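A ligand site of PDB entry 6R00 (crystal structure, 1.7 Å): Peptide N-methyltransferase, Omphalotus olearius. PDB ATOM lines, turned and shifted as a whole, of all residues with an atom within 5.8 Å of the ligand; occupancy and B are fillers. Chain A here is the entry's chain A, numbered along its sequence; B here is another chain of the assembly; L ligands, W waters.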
ATOM      1  N   ILE A  18       4.771   9.429 -10.048  1.00  0.00           N
ATOM      2  CA  ILE A  18       6.136   9.957  -9.790  1.00  0.00           C
ATOM      3  C   ILE A  18       6.320  11.277 -10.521  1.00  0.00           C
ATOM      4  O   ILE A  18       6.759  12.275  -9.897  1.00  0.00           O
ATOM      5  CB  ILE A  18       7.185   8.910 -10.163  1.00  0.00           C
ATOM      6  CG1 ILE A  18       7.063   7.641  -9.311  1.00  0.00           C
ATOM      7  CG2 ILE A  18       8.574   9.525 -10.074  1.00  0.00           C
ATOM      8  CD1 ILE A  18       7.296   7.830  -7.832  1.00  0.00           C
ATOM      9  N   ILE A  43       6.492  14.887  -3.522  1.00  0.00           N
ATOM     10  CA  ILE A  43       7.901  15.360  -3.616  1.00  0.00           C
ATOM     11  C   ILE A  43       7.949  16.745  -4.247  1.00  0.00           C
ATOM     12  O   ILE A  43       8.673  17.654  -3.710  1.00  0.00           O
ATOM     13  CB  ILE A  43       8.812  14.356  -4.340  1.00  0.00           C
ATOM     14  CG1 ILE A  43       8.943  13.060  -3.520  1.00  0.00           C
ATOM     15  CG2 ILE A  43      10.159  15.014  -4.589  1.00  0.00           C
ATOM     16  CD1 ILE A  43       9.957  12.104  -4.074  1.00  0.00           C
ATOM     17  N   TYR A  97       3.007  10.202  -2.740  1.00  0.00           N
ATOM     18  CA  TYR A  97       3.518  10.154  -4.108  1.00  0.00           C
ATOM     19  C   TYR A  97       3.740   8.707  -4.550  1.00  0.00           C
ATOM     20  O   TYR A  97       3.927   7.785  -3.724  1.00  0.00           O
ATOM     21  CB  TYR A  97       4.740  11.016  -4.253  1.00  0.00           C
ATOM     22  CG  TYR A  97       5.956  10.454  -3.639  1.00  0.00           C
ATOM     23  CD1 TYR A  97       6.219  10.582  -2.285  1.00  0.00           C
ATOM     24  CD2 TYR A  97       6.846   9.740  -4.422  1.00  0.00           C
ATOM     25  CE1 TYR A  97       7.390  10.079  -1.739  1.00  0.00           C
ATOM     26  CE2 TYR A  97       7.993   9.210  -3.902  1.00  0.00           C
ATOM     27  CZ  TYR A  97       8.276   9.364  -2.555  1.00  0.00           C
ATOM     28  OH  TYR A  97       9.452   8.868  -2.037  1.00  0.00           O
ATOM     29  N   GLY A  98       3.735   8.544  -5.863  1.00  0.00           N
ATOM     30  CA  GLY A  98       3.863   7.213  -6.474  1.00  0.00           C
ATOM     31  C   GLY A  98       2.608   6.400  -6.267  1.00  0.00           C
ATOM     32  O   GLY A  98       1.487   6.924  -6.464  1.00  0.00           O
ATOM     33  N   HIS A  99       2.783   5.153  -5.878  1.00  0.00           N
ATOM     34  CA  HIS A  99       1.720   4.257  -5.404  1.00  0.00           C
ATOM     35  C   HIS A  99       1.702   4.383  -3.891  1.00  0.00           C
ATOM     36  O   HIS A  99       2.750   4.235  -3.264  1.00  0.00           O
ATOM     37  CB  HIS A  99       2.044   2.832  -5.823  1.00  0.00           C
ATOM     38  CG  HIS A  99       1.033   1.810  -5.479  1.00  0.00           C
ATOM     39  ND1 HIS A  99       0.527   1.663  -4.192  1.00  0.00           N
ATOM     40  CD2 HIS A  99       0.474   0.830  -6.235  1.00  0.00           C
ATOM     41  CE1 HIS A  99      -0.299   0.641  -4.169  1.00  0.00           C
ATOM     42  NE2 HIS A  99      -0.323   0.069  -5.409  1.00  0.00           N
ATOM     43  N   PRO A 100       0.549   4.692  -3.269  1.00  0.00           N
ATOM     44  CA  PRO A 100       0.555   5.066  -1.849  1.00  0.00           C
ATOM     45  C   PRO A 100       0.755   3.883  -0.897  1.00  0.00           C
ATOM     46  O   PRO A 100       0.814   4.094   0.285  1.00  0.00           O
ATOM     47  CB  PRO A 100      -0.843   5.681  -1.707  1.00  0.00           C
ATOM     48  CG  PRO A 100      -1.699   4.874  -2.663  1.00  0.00           C
ATOM     49  CD  PRO A 100      -0.800   4.731  -3.883  1.00  0.00           C
ATOM     50  N   GLY A 101       0.840   2.651  -1.435  1.00  0.00           N
ATOM     51  CA  GLY A 101       1.075   1.440  -0.639  1.00  0.00           C
ATOM     52  C   GLY A 101       2.418   0.773  -0.914  1.00  0.00           C
ATOM     53  O   GLY A 101       2.629  -0.325  -0.370  1.00  0.00           O
ATOM     54  N   VAL A 102       3.249   1.372  -1.754  1.00  0.00           N
ATOM     55  CA  VAL A 102       4.559   0.801  -2.200  1.00  0.00           C
ATOM     56  C   VAL A 102       5.659   1.542  -1.475  1.00  0.00           C
ATOM     57  O   VAL A 102       5.856   2.752  -1.709  1.00  0.00           O
ATOM     58  CB  VAL A 102       4.660   0.860  -3.740  1.00  0.00           C
ATOM     59  CG1 VAL A 102       6.064   0.612  -4.256  1.00  0.00           C
ATOM     60  CG2 VAL A 102       3.667  -0.087  -4.391  1.00  0.00           C
ATOM     61  N   PHE A 103       6.274   0.868  -0.511  1.00  0.00           N
ATOM     62  CA  PHE A 103       7.296   1.447   0.367  1.00  0.00           C
ATOM     63  C   PHE A 103       6.681   2.659   1.107  1.00  0.00           C
ATOM     64  O   PHE A 103       7.283   3.739   1.104  1.00  0.00           O
ATOM     65  CB  PHE A 103       8.562   1.819  -0.428  1.00  0.00           C
ATOM     66  CG  PHE A 103       9.250   0.614  -1.050  1.00  0.00           C
ATOM     67  CD1 PHE A 103       8.739   0.005  -2.192  1.00  0.00           C
ATOM     68  CD2 PHE A 103      10.351   0.038  -0.449  1.00  0.00           C
ATOM     69  CE1 PHE A 103       9.335  -1.134  -2.724  1.00  0.00           C
ATOM     70  CE2 PHE A 103      10.921  -1.119  -0.977  1.00  0.00           C
ATOM     71  CZ  PHE A 103      10.427  -1.689  -2.120  1.00  0.00           C
ATOM     72  N   VAL A 104       5.482   2.502   1.666  1.00  0.00           N
ATOM     73  CA  VAL A 104       4.828   3.553   2.514  1.00  0.00           C
ATOM     74  C   VAL A 104       4.277   2.893   3.786  1.00  0.00           C
ATOM     75  O   VAL A 104       3.417   2.039   3.691  1.00  0.00           O
ATOM     76  CB  VAL A 104       3.695   4.280   1.780  1.00  0.00           C
ATOM     77  CG1 VAL A 104       3.096   5.376   2.638  1.00  0.00           C
ATOM     78  CG2 VAL A 104       4.136   4.871   0.444  1.00  0.00           C
ATOM     79  N   VAL A 127       0.880   4.824  -9.887  1.00  0.00           N
ATOM     80  CA  VAL A 127       2.125   4.529 -10.630  1.00  0.00           C
ATOM     81  C   VAL A 127       3.319   4.649  -9.684  1.00  0.00           C
ATOM     82  O   VAL A 127       3.588   5.759  -9.185  1.00  0.00           O
ATOM     83  CB  VAL A 127       2.249   5.484 -11.812  1.00  0.00           C
ATOM     84  CG1 VAL A 127       3.596   5.319 -12.486  1.00  0.00           C
ATOM     85  CG2 VAL A 127       1.085   5.251 -12.774  1.00  0.00           C
ATOM     86  N   SER A 128       3.997   3.543  -9.464  1.00  0.00           N
ATOM     87  CA  SER A 128       5.181   3.487  -8.583  1.00  0.00           C
ATOM     88  C   SER A 128       6.461   3.856  -9.309  1.00  0.00           C
ATOM     89  O   SER A 128       6.531   3.894 -10.552  1.00  0.00           O
ATOM     90  CB  SER A 128       5.319   2.154  -7.953  1.00  0.00           C
ATOM     91  OG  SER A 128       5.826   1.214  -8.908  1.00  0.00           O
ATOM     92  N   ALA A 129       7.524   4.060  -8.540  1.00  0.00           N
ATOM     93  CA  ALA A 129       8.875   4.241  -9.101  1.00  0.00           C
ATOM     94  C   ALA A 129       9.281   3.005  -9.896  1.00  0.00           C
ATOM     95  O   ALA A 129      10.015   3.155 -10.900  1.00  0.00           O
ATOM     96  CB  ALA A 129       9.864   4.551  -8.024  1.00  0.00           C
ATOM     97  N   GLU A 130       8.837   1.821  -9.502  1.00  0.00           N
ATOM     98  CA  GLU A 130       9.167   0.567 -10.224  1.00  0.00           C
ATOM     99  C   GLU A 130       8.411   0.578 -11.562  1.00  0.00           C
ATOM    100  O   GLU A 130       9.016   0.192 -12.572  1.00  0.00           O
ATOM    101  CB  GLU A 130       8.827  -0.655  -9.393  1.00  0.00           C
ATOM    102  CG  GLU A 130       9.214  -1.924 -10.097  1.00  0.00           C
ATOM    103  CD  GLU A 130       9.161  -3.137  -9.198  1.00  0.00           C
ATOM    104  OE1 GLU A 130       8.097  -3.720  -9.054  1.00  0.00           O
ATOM    105  OE2 GLU A 130      10.222  -3.476  -8.657  1.00  0.00           O
ATOM    106  N   LEU A 169      16.150  -2.518  -6.358  1.00  0.00           N
ATOM    107  CA  LEU A 169      16.392  -2.097  -4.947  1.00  0.00           C
ATOM    108  C   LEU A 169      15.963  -0.645  -4.739  1.00  0.00           C
ATOM    109  O   LEU A 169      16.540   0.246  -5.388  1.00  0.00           O
ATOM    110  CB  LEU A 169      17.888  -2.267  -4.645  1.00  0.00           C
ATOM    111  CG  LEU A 169      18.437  -3.693  -4.675  1.00  0.00           C
ATOM    112  CD1 LEU A 169      19.916  -3.681  -4.304  1.00  0.00           C
ATOM    113  CD2 LEU A 169      17.684  -4.601  -3.733  1.00  0.00           C
ATOM    114  N   PHE A 170      15.015  -0.421  -3.806  1.00  0.00           N
ATOM    115  CA  PHE A 170      14.510   0.908  -3.375  1.00  0.00           C
ATOM    116  C   PHE A 170      15.298   1.383  -2.144  1.00  0.00           C
ATOM    117  O   PHE A 170      15.817   0.537  -1.377  1.00  0.00           O
ATOM    118  CB  PHE A 170      13.044   0.864  -2.954  1.00  0.00           C
ATOM    119  CG  PHE A 170      12.002   0.884  -4.058  1.00  0.00           C
ATOM    120  CD1 PHE A 170      11.891  -0.186  -4.928  1.00  0.00           C
ATOM    121  CD2 PHE A 170      11.091   1.917  -4.126  1.00  0.00           C
ATOM    122  CE1 PHE A 170      10.909  -0.177  -5.934  1.00  0.00           C
ATOM    123  CE2 PHE A 170      10.121   1.939  -5.120  1.00  0.00           C
ATOM    124  CZ  PHE A 170      10.039   0.890  -6.031  1.00  0.00           C
ATOM    125  N   GLN A 171      15.344   2.697  -1.912  1.00  0.00           N
ATOM    126  CA  GLN A 171      15.901   3.295  -0.647  1.00  0.00           C
ATOM    127  C   GLN A 171      17.377   2.942  -0.554  1.00  0.00           C
ATOM    128  O   GLN A 171      17.916   2.811   0.586  1.00  0.00           O
ATOM    129  CB  GLN A 171      15.096   2.884   0.584  1.00  0.00           C
ATOM    130  CG  GLN A 171      13.632   3.251   0.434  1.00  0.00           C
ATOM    131  CD  GLN A 171      12.853   3.626   1.675  1.00  0.00           C
ATOM    132  OE1 GLN A 171      11.899   4.409   1.589  1.00  0.00           O
ATOM    133  NE2 GLN A 171      13.203   3.017   2.805  1.00  0.00           N
ATOM    134  N   VAL A 172      18.067   2.959  -1.686  1.00  0.00           N
ATOM    135  CA  VAL A 172      19.528   2.715  -1.694  1.00  0.00           C
ATOM    136  C   VAL A 172      20.262   3.968  -1.172  1.00  0.00           C
ATOM    137  O   VAL A 172      21.468   3.830  -0.854  1.00  0.00           O
ATOM    138  CB  VAL A 172      20.053   2.318  -3.074  1.00  0.00           C
ATOM    139  CG1 VAL A 172      19.603   0.908  -3.473  1.00  0.00           C
ATOM    140  CG2 VAL A 172      19.638   3.297  -4.167  1.00  0.00           C
ATOM    141  N   GLY A 173      19.611   5.139  -1.085  1.00  0.00           N
ATOM    142  CA  GLY A 173      20.285   6.347  -0.559  1.00  0.00           C
ATOM    143  C   GLY A 173      20.219   6.490   0.956  1.00  0.00           C
ATOM    144  O   GLY A 173      20.685   7.529   1.459  1.00  0.00           O
ATOM    145  N   CYS A 174      19.600   5.566   1.679  1.00  0.00           N
ATOM    146  CA  CYS A 174      19.478   5.666   3.160  1.00  0.00           C
ATOM    147  C   CYS A 174      19.682   4.298   3.805  1.00  0.00           C
ATOM    148  O   CYS A 174      18.950   3.950   4.765  1.00  0.00           O
ATOM    149  CB  CYS A 174      18.179   6.356   3.587  1.00  0.00           C
ATOM    150  SG  CYS A 174      16.667   5.591   2.946  1.00  0.00           S
ATOM    151  N   TYR A 210      18.956   4.572 -11.423  1.00  0.00           N
ATOM    152  CA  TYR A 210      17.693   5.041 -12.011  1.00  0.00           C
ATOM    153  C   TYR A 210      17.083   6.153 -11.159  1.00  0.00           C
ATOM    154  O   TYR A 210      16.796   5.978  -9.943  1.00  0.00           O
ATOM    155  CB  TYR A 210      16.732   3.859 -12.217  1.00  0.00           C
ATOM    156  CG  TYR A 210      15.422   4.323 -12.756  1.00  0.00           C
ATOM    157  CD1 TYR A 210      15.363   4.895 -14.025  1.00  0.00           C
ATOM    158  CD2 TYR A 210      14.251   4.238 -12.022  1.00  0.00           C
ATOM    159  CE1 TYR A 210      14.165   5.382 -14.522  1.00  0.00           C
ATOM    160  CE2 TYR A 210      13.047   4.725 -12.506  1.00  0.00           C
ATOM    161  CZ  TYR A 210      13.003   5.298 -13.767  1.00  0.00           C
ATOM    162  OH  TYR A 210      11.839   5.757 -14.303  1.00  0.00           O
ATOM    163  N   ILE A 211      16.824   7.291 -11.818  1.00  0.00           N
ATOM    164  CA  ILE A 211      15.952   8.341 -11.232  1.00  0.00           C
ATOM    165  C   ILE A 211      14.963   8.747 -12.324  1.00  0.00           C
ATOM    166  O   ILE A 211      15.378   9.229 -13.399  1.00  0.00           O
ATOM    167  CB  ILE A 211      16.706   9.561 -10.662  1.00  0.00           C
ATOM    168  CG1 ILE A 211      17.836   9.143  -9.723  1.00  0.00           C
ATOM    169  CG2 ILE A 211      15.696  10.466  -9.966  1.00  0.00           C
ATOM    170  CD1 ILE A 211      18.721  10.282  -9.255  1.00  0.00           C
ATOM    171  N   ALA A 212      13.705   8.419 -12.077  1.00  0.00           N
ATOM    172  CA  ALA A 212      12.569   8.829 -12.917  1.00  0.00           C
ATOM    173  C   ALA A 212      12.523  10.359 -12.909  1.00  0.00           C
ATOM    174  O   ALA A 212      12.666  10.953 -11.825  1.00  0.00           O
ATOM    175  CB  ALA A 212      11.301   8.227 -12.392  1.00  0.00           C
ATOM    176  N   ALA A 213      12.246  10.948 -14.067  1.00  0.00           N
ATOM    177  CA  ALA A 213      12.007  12.399 -14.192  1.00  0.00           C
ATOM    178  C   ALA A 213      10.834  12.769 -13.285  1.00  0.00           C
ATOM    179  O   ALA A 213       9.772  12.095 -13.326  1.00  0.00           O
ATOM    180  CB  ALA A 213      11.735  12.766 -15.649  1.00  0.00           C
ATOM    181  N   MET A 214      11.011  13.804 -12.470  1.00  0.00           N
ATOM    182  CA  MET A 214       9.894  14.246 -11.593  1.00  0.00           C
ATOM    183  C   MET A 214       9.185  15.441 -12.224  1.00  0.00           C
ATOM    184  O   MET A 214       8.029  15.683 -11.891  1.00  0.00           O
ATOM    185  CB  MET A 214      10.441  14.542 -10.197  1.00  0.00           C
ATOM    186  CG  MET A 214      10.554  13.233  -9.447  1.00  0.00           C
ATOM    187  SD  MET A 214      11.528  13.340  -7.956  1.00  0.00           S
ATOM    188  CE  MET A 214      13.166  13.670  -8.606  1.00  0.00           C
ATOM    189  N   GLY A 240      20.909   9.383  -4.023  1.00  0.00           N
ATOM    190  CA  GLY A 240      20.104  10.168  -3.077  1.00  0.00           C
ATOM    191  C   GLY A 240      18.785   9.538  -2.700  1.00  0.00           C
ATOM    192  O   GLY A 240      18.590   8.336  -2.922  1.00  0.00           O
ATOM    193  N   GLY A 241      17.890  10.354  -2.168  1.00  0.00           N
ATOM    194  CA  GLY A 241      16.593   9.949  -1.580  1.00  0.00           C
ATOM    195  C   GLY A 241      15.629   9.438  -2.612  1.00  0.00           C
ATOM    196  O   GLY A 241      14.616   8.821  -2.196  1.00  0.00           O
ATOM    197  N   VAL A 242      15.870   9.708  -3.904  1.00  0.00           N
ATOM    198  CA  VAL A 242      14.927   9.249  -4.980  1.00  0.00           C
ATOM    199  C   VAL A 242      15.664   8.298  -5.947  1.00  0.00           C
ATOM    200  O   VAL A 242      15.159   8.076  -7.045  1.00  0.00           O
ATOM    201  CB  VAL A 242      14.259  10.421  -5.725  1.00  0.00           C
ATOM    202  CG1 VAL A 242      13.257  11.131  -4.822  1.00  0.00           C
ATOM    203  CG2 VAL A 242      15.271  11.377  -6.324  1.00  0.00           C
ATOM    204  N   SER A 243      16.828   7.782  -5.567  1.00  0.00           N
ATOM    205  CA  SER A 243      17.633   6.820  -6.347  1.00  0.00           C
ATOM    206  C   SER A 243      17.106   5.387  -6.136  1.00  0.00           C
ATOM    207  O   SER A 243      16.838   4.977  -4.995  1.00  0.00           O
ATOM    208  CB  SER A 243      19.080   6.891  -6.001  1.00  0.00           C
ATOM    209  OG  SER A 243      19.607   8.186  -6.265  1.00  0.00           O
ATOM    210  N   THR A 244      16.983   4.671  -7.241  1.00  0.00           N
ATOM    211  CA  THR A 244      16.614   3.240  -7.253  1.00  0.00           C
ATOM    212  C   THR A 244      17.705   2.545  -8.046  1.00  0.00           C
ATOM    213  O   THR A 244      18.211   3.136  -8.980  1.00  0.00           O
ATOM    214  CB  THR A 244      15.220   3.031  -7.838  1.00  0.00           C
ATOM    215  OG1 THR A 244      14.306   3.598  -6.901  1.00  0.00           O
ATOM    216  CG2 THR A 244      14.881   1.569  -8.038  1.00  0.00           C
ATOM    217  N   MVA B   4      12.014  12.154   0.653  1.00  0.00           N
ATOM    218  CN  MVA B   4      12.427  11.441  -0.565  1.00  0.00           C
ATOM    219  CA  MVA B   4      10.655  11.868   1.157  1.00  0.00           C
ATOM    220  CB  MVA B   4       9.549  12.467   0.266  1.00  0.00           C
ATOM    221  CG1 MVA B   4       9.868  13.907  -0.133  1.00  0.00           C
ATOM    222  CG2 MVA B   4       8.189  12.399   0.976  1.00  0.00           C
ATOM    223  C   MVA B   4      10.536  10.366   1.322  1.00  0.00           C
ATOM    224  O   MVA B   4      10.048   9.624   0.455  1.00  0.00           O
ATOM    225  N   ILE B   5      11.104   9.921   2.440  1.00  0.00           N
ATOM    226  CA  ILE B   5      11.196   8.511   2.739  1.00  0.00           C
ATOM    227  C   ILE B   5       9.998   8.151   3.604  1.00  0.00           C
ATOM    228  O   ILE B   5       9.894   8.671   4.716  1.00  0.00           O
ATOM    229  CB  ILE B   5      12.538   8.238   3.446  1.00  0.00           C
ATOM    230  CG1 ILE B   5      13.712   8.636   2.554  1.00  0.00           C
ATOM    231  CG2 ILE B   5      12.619   6.798   3.903  1.00  0.00           C
ATOM    232  CD1 ILE B   5      13.735   7.895   1.221  1.00  0.00           C
ATOM    233  N   MVA B   6       9.081   7.288   3.134  1.00  0.00           N
ATOM    234  CN  MVA B   6       9.190   6.486   1.918  1.00  0.00           C
ATOM    235  CA  MVA B   6       7.832   7.126   3.927  1.00  0.00           C
ATOM    236  CB  MVA B   6       6.568   7.621   3.198  1.00  0.00           C
ATOM    237  CG1 MVA B   6       5.542   8.150   4.194  1.00  0.00           C
ATOM    238  CG2 MVA B   6       6.848   8.688   2.140  1.00  0.00           C
ATOM    239  C   MVA B   6       7.752   5.682   4.388  1.00  0.00           C
ATOM    240  O   MVA B   6       6.688   5.162   4.671  1.00  0.00           O
ATOM    241  N   PHE B   7       8.933   5.060   4.474  1.00  0.00           N
ATOM    242  CA  PHE B   7       9.053   3.679   4.902  1.00  0.00           C
ATOM    243  C   PHE B   7      10.383   3.471   5.634  1.00  0.00           C
ATOM    244  O   PHE B   7      11.397   4.087   5.288  1.00  0.00           O
ATOM    245  CB  PHE B   7       8.946   2.761   3.683  1.00  0.00           C
ATOM    246  CG  PHE B   7       9.010   1.299   4.039  1.00  0.00           C
ATOM    247  CD1 PHE B   7       7.884   0.661   4.528  1.00  0.00           C
ATOM    248  CD2 PHE B   7      10.191   0.592   3.893  1.00  0.00           C
ATOM    249  CE1 PHE B   7       7.943  -0.692   4.873  1.00  0.00           C
ATOM    250  CE2 PHE B   7      10.252  -0.756   4.247  1.00  0.00           C
ATOM    251  CZ  PHE B   7       9.119  -1.386   4.733  1.00  0.00           C
HETATM  252  N1  LIG L   1       5.513   5.139  -2.872  1.00  0.00           N
HETATM  253  C1  LIG L   1       6.700   5.417  -3.725  1.00  0.00           C
HETATM  254  C2  LIG L   1       7.993   4.937  -3.046  1.00  0.00           C
HETATM  255  C3  LIG L   1       8.227   5.580  -1.696  1.00  0.00           C
HETATM  256  S1  LIG L   1       9.719   4.950  -0.877  1.00  0.00           S
HETATM  257  C4  LIG L   1       6.535   4.678  -5.051  1.00  0.00           C
HETATM  258  O1  LIG L   1       7.537   4.492  -5.773  1.00  0.00           O
HETATM  259  O2  LIG L   1       5.433   4.300  -5.346  1.00  0.00           O
HETATM  260  C5  LIG L   1      11.050   5.947  -1.572  1.00  0.00           C
HETATM  261  C6  LIG L   1      11.930   5.234  -2.585  1.00  0.00           C
HETATM  262  O3  LIG L   1      11.241   5.187  -3.862  1.00  0.00           O
HETATM  263  C7  LIG L   1      13.240   5.927  -2.914  1.00  0.00           C
HETATM  264  O4  LIG L   1      14.259   5.689  -1.966  1.00  0.00           O
HETATM  265  C8  LIG L   1      13.571   5.307  -4.279  1.00  0.00           C
HETATM  266  O5  LIG L   1      14.118   4.005  -4.179  1.00  0.00           O
HETATM  267  C9  LIG L   1      12.181   5.269  -4.911  1.00  0.00           C
HETATM  268  N2  LIG L   1      11.925   6.479  -5.702  1.00  0.00           N
HETATM  269  C10 LIG L   1      11.219   7.593  -5.329  1.00  0.00           C
HETATM  270  N3  LIG L   1      11.202   8.538  -6.240  1.00  0.00           N
HETATM  271  C11 LIG L   1      11.946   8.009  -7.287  1.00  0.00           C
HETATM  272  C12 LIG L   1      12.292   8.510  -8.564  1.00  0.00           C
HETATM  273  N4  LIG L   1      11.987   9.728  -9.012  1.00  0.00           N
HETATM  274  N5  LIG L   1      13.039   7.711  -9.350  1.00  0.00           N
HETATM  275  C13 LIG L   1      13.415   6.511  -8.893  1.00  0.00           C
HETATM  276  N6  LIG L   1      13.164   5.939  -7.727  1.00  0.00           N
HETATM  277  C14 LIG L   1      12.399   6.739  -6.973  1.00  0.00           C
HETATM  278  O   HOH W   1       5.092   7.601  -1.413  1.00  0.00           O
HETATM  279  O   HOH W   2      17.122   5.988  -2.406  1.00  0.00           O
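Water W1 lies within hydrogen-bond range of O of Tyr 97 (2.6 Å) and N1 of the ligand (2.9 Å).
Water W2 lies within hydrogen-bond range of the backbone carbonyl oxygen (O) of Ser 243 (2.8 Å), the backbone carbonyl oxygen (O) of Gly 240 (2.8 Å), an oxygen (O4) of the ligand (2.9 Å), the backbone NH (N) of Gly 173 (2.9 Å) and the backbone NH (N) of Val 172 (3.3 Å).
O of Phe 103 sits close to S1 of the ligand (3.4 Å).
A nitrogen (N6) of the ligand sits close to the backbone carbonyl oxygen of Val 242 (3.0 Å).
Merely in contact with the ligand: Phe 170 (3.2 Å), MVA 6 of chain B (3.2 Å), Ser 128 (3.3 Å), Gly 98 (3.5 Å), Ile 211 (3.5 Å), Ile 18 (3.6 Å), Tyr 210 (3.6 Å), Val 104 (3.6 Å) and Ile 5 of chain B (3.9 Å).
Of the 34 residues printed, 21 come within 4 Å of the ligand.
O of Val 102 sits at hydrogen-bond distance from N1 of the ligand (2.7 Å).
The side-chain hydroxyl (OG1) of Thr 244 sits at hydrogen-bond distance from a nitrogen (N6) of the ligand.
O1 of the ligand lies within hydrogen-bond range of N of Ala 129.
N of His 99 sits at hydrogen-bond distance from O2 of the ligand, 2.8 Å away.
O of His 99 lies within hydrogen-bond range of N1 of the ligand.
An oxygen (O5) of the ligand is in hydrogen-bond range of the backbone NH of Gln 171 (2.9 Å).
The side-chain amide oxygen (OE1) of Gln 171 lies close to a sulfur (S1) of the ligand.
N of Ala 212 is in hydrogen-bond range of N5 of the ligand (2.9 Å).
The backbone carbonyl oxygen (O) of Ala 212 lies within hydrogen-bond range of a nitrogen (N4) of the ligand.
An oxygen (O5) of the ligand lies within hydrogen-bond range of the backbone carbonyl oxygen of Ser 243 (3.0 Å).
O of Gly 241 sits at hydrogen-bond distance from O4 of the ligand (3.2 Å).
O of Tyr 97 is in hydrogen-bond range of N1 of the ligand, 3.2 Å away.
SD of Met 214 is in hydrogen-bond range of N4 of the ligand (3.8 Å).
N of Tyr 210 lies within hydrogen-bond range of O of Thr 244 (2.9 Å).
N of His 99 sits at hydrogen-bond distance from O of Val 127 (3.5 Å).
The backbone NH (N) of Gly 101 is in hydrogen-bond range of a ring nitrogen (ND1) of His 99 (2.9 Å).
NE2 of Gln 171 is in hydrogen-bond range of O of Phe 7 of chain B (3.3 Å).
N of Gly 240 sits at hydrogen-bond distance from OG of Ser 243 (2.9 Å).
O of MVA 4 of chain B sits at hydrogen-bond distance from OH of Tyr 97 (2.7 Å).
The side-chain hydroxyl of Ser 128 is in hydrogen-bond range of the backbone NH of Glu 130 (3.1 Å).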
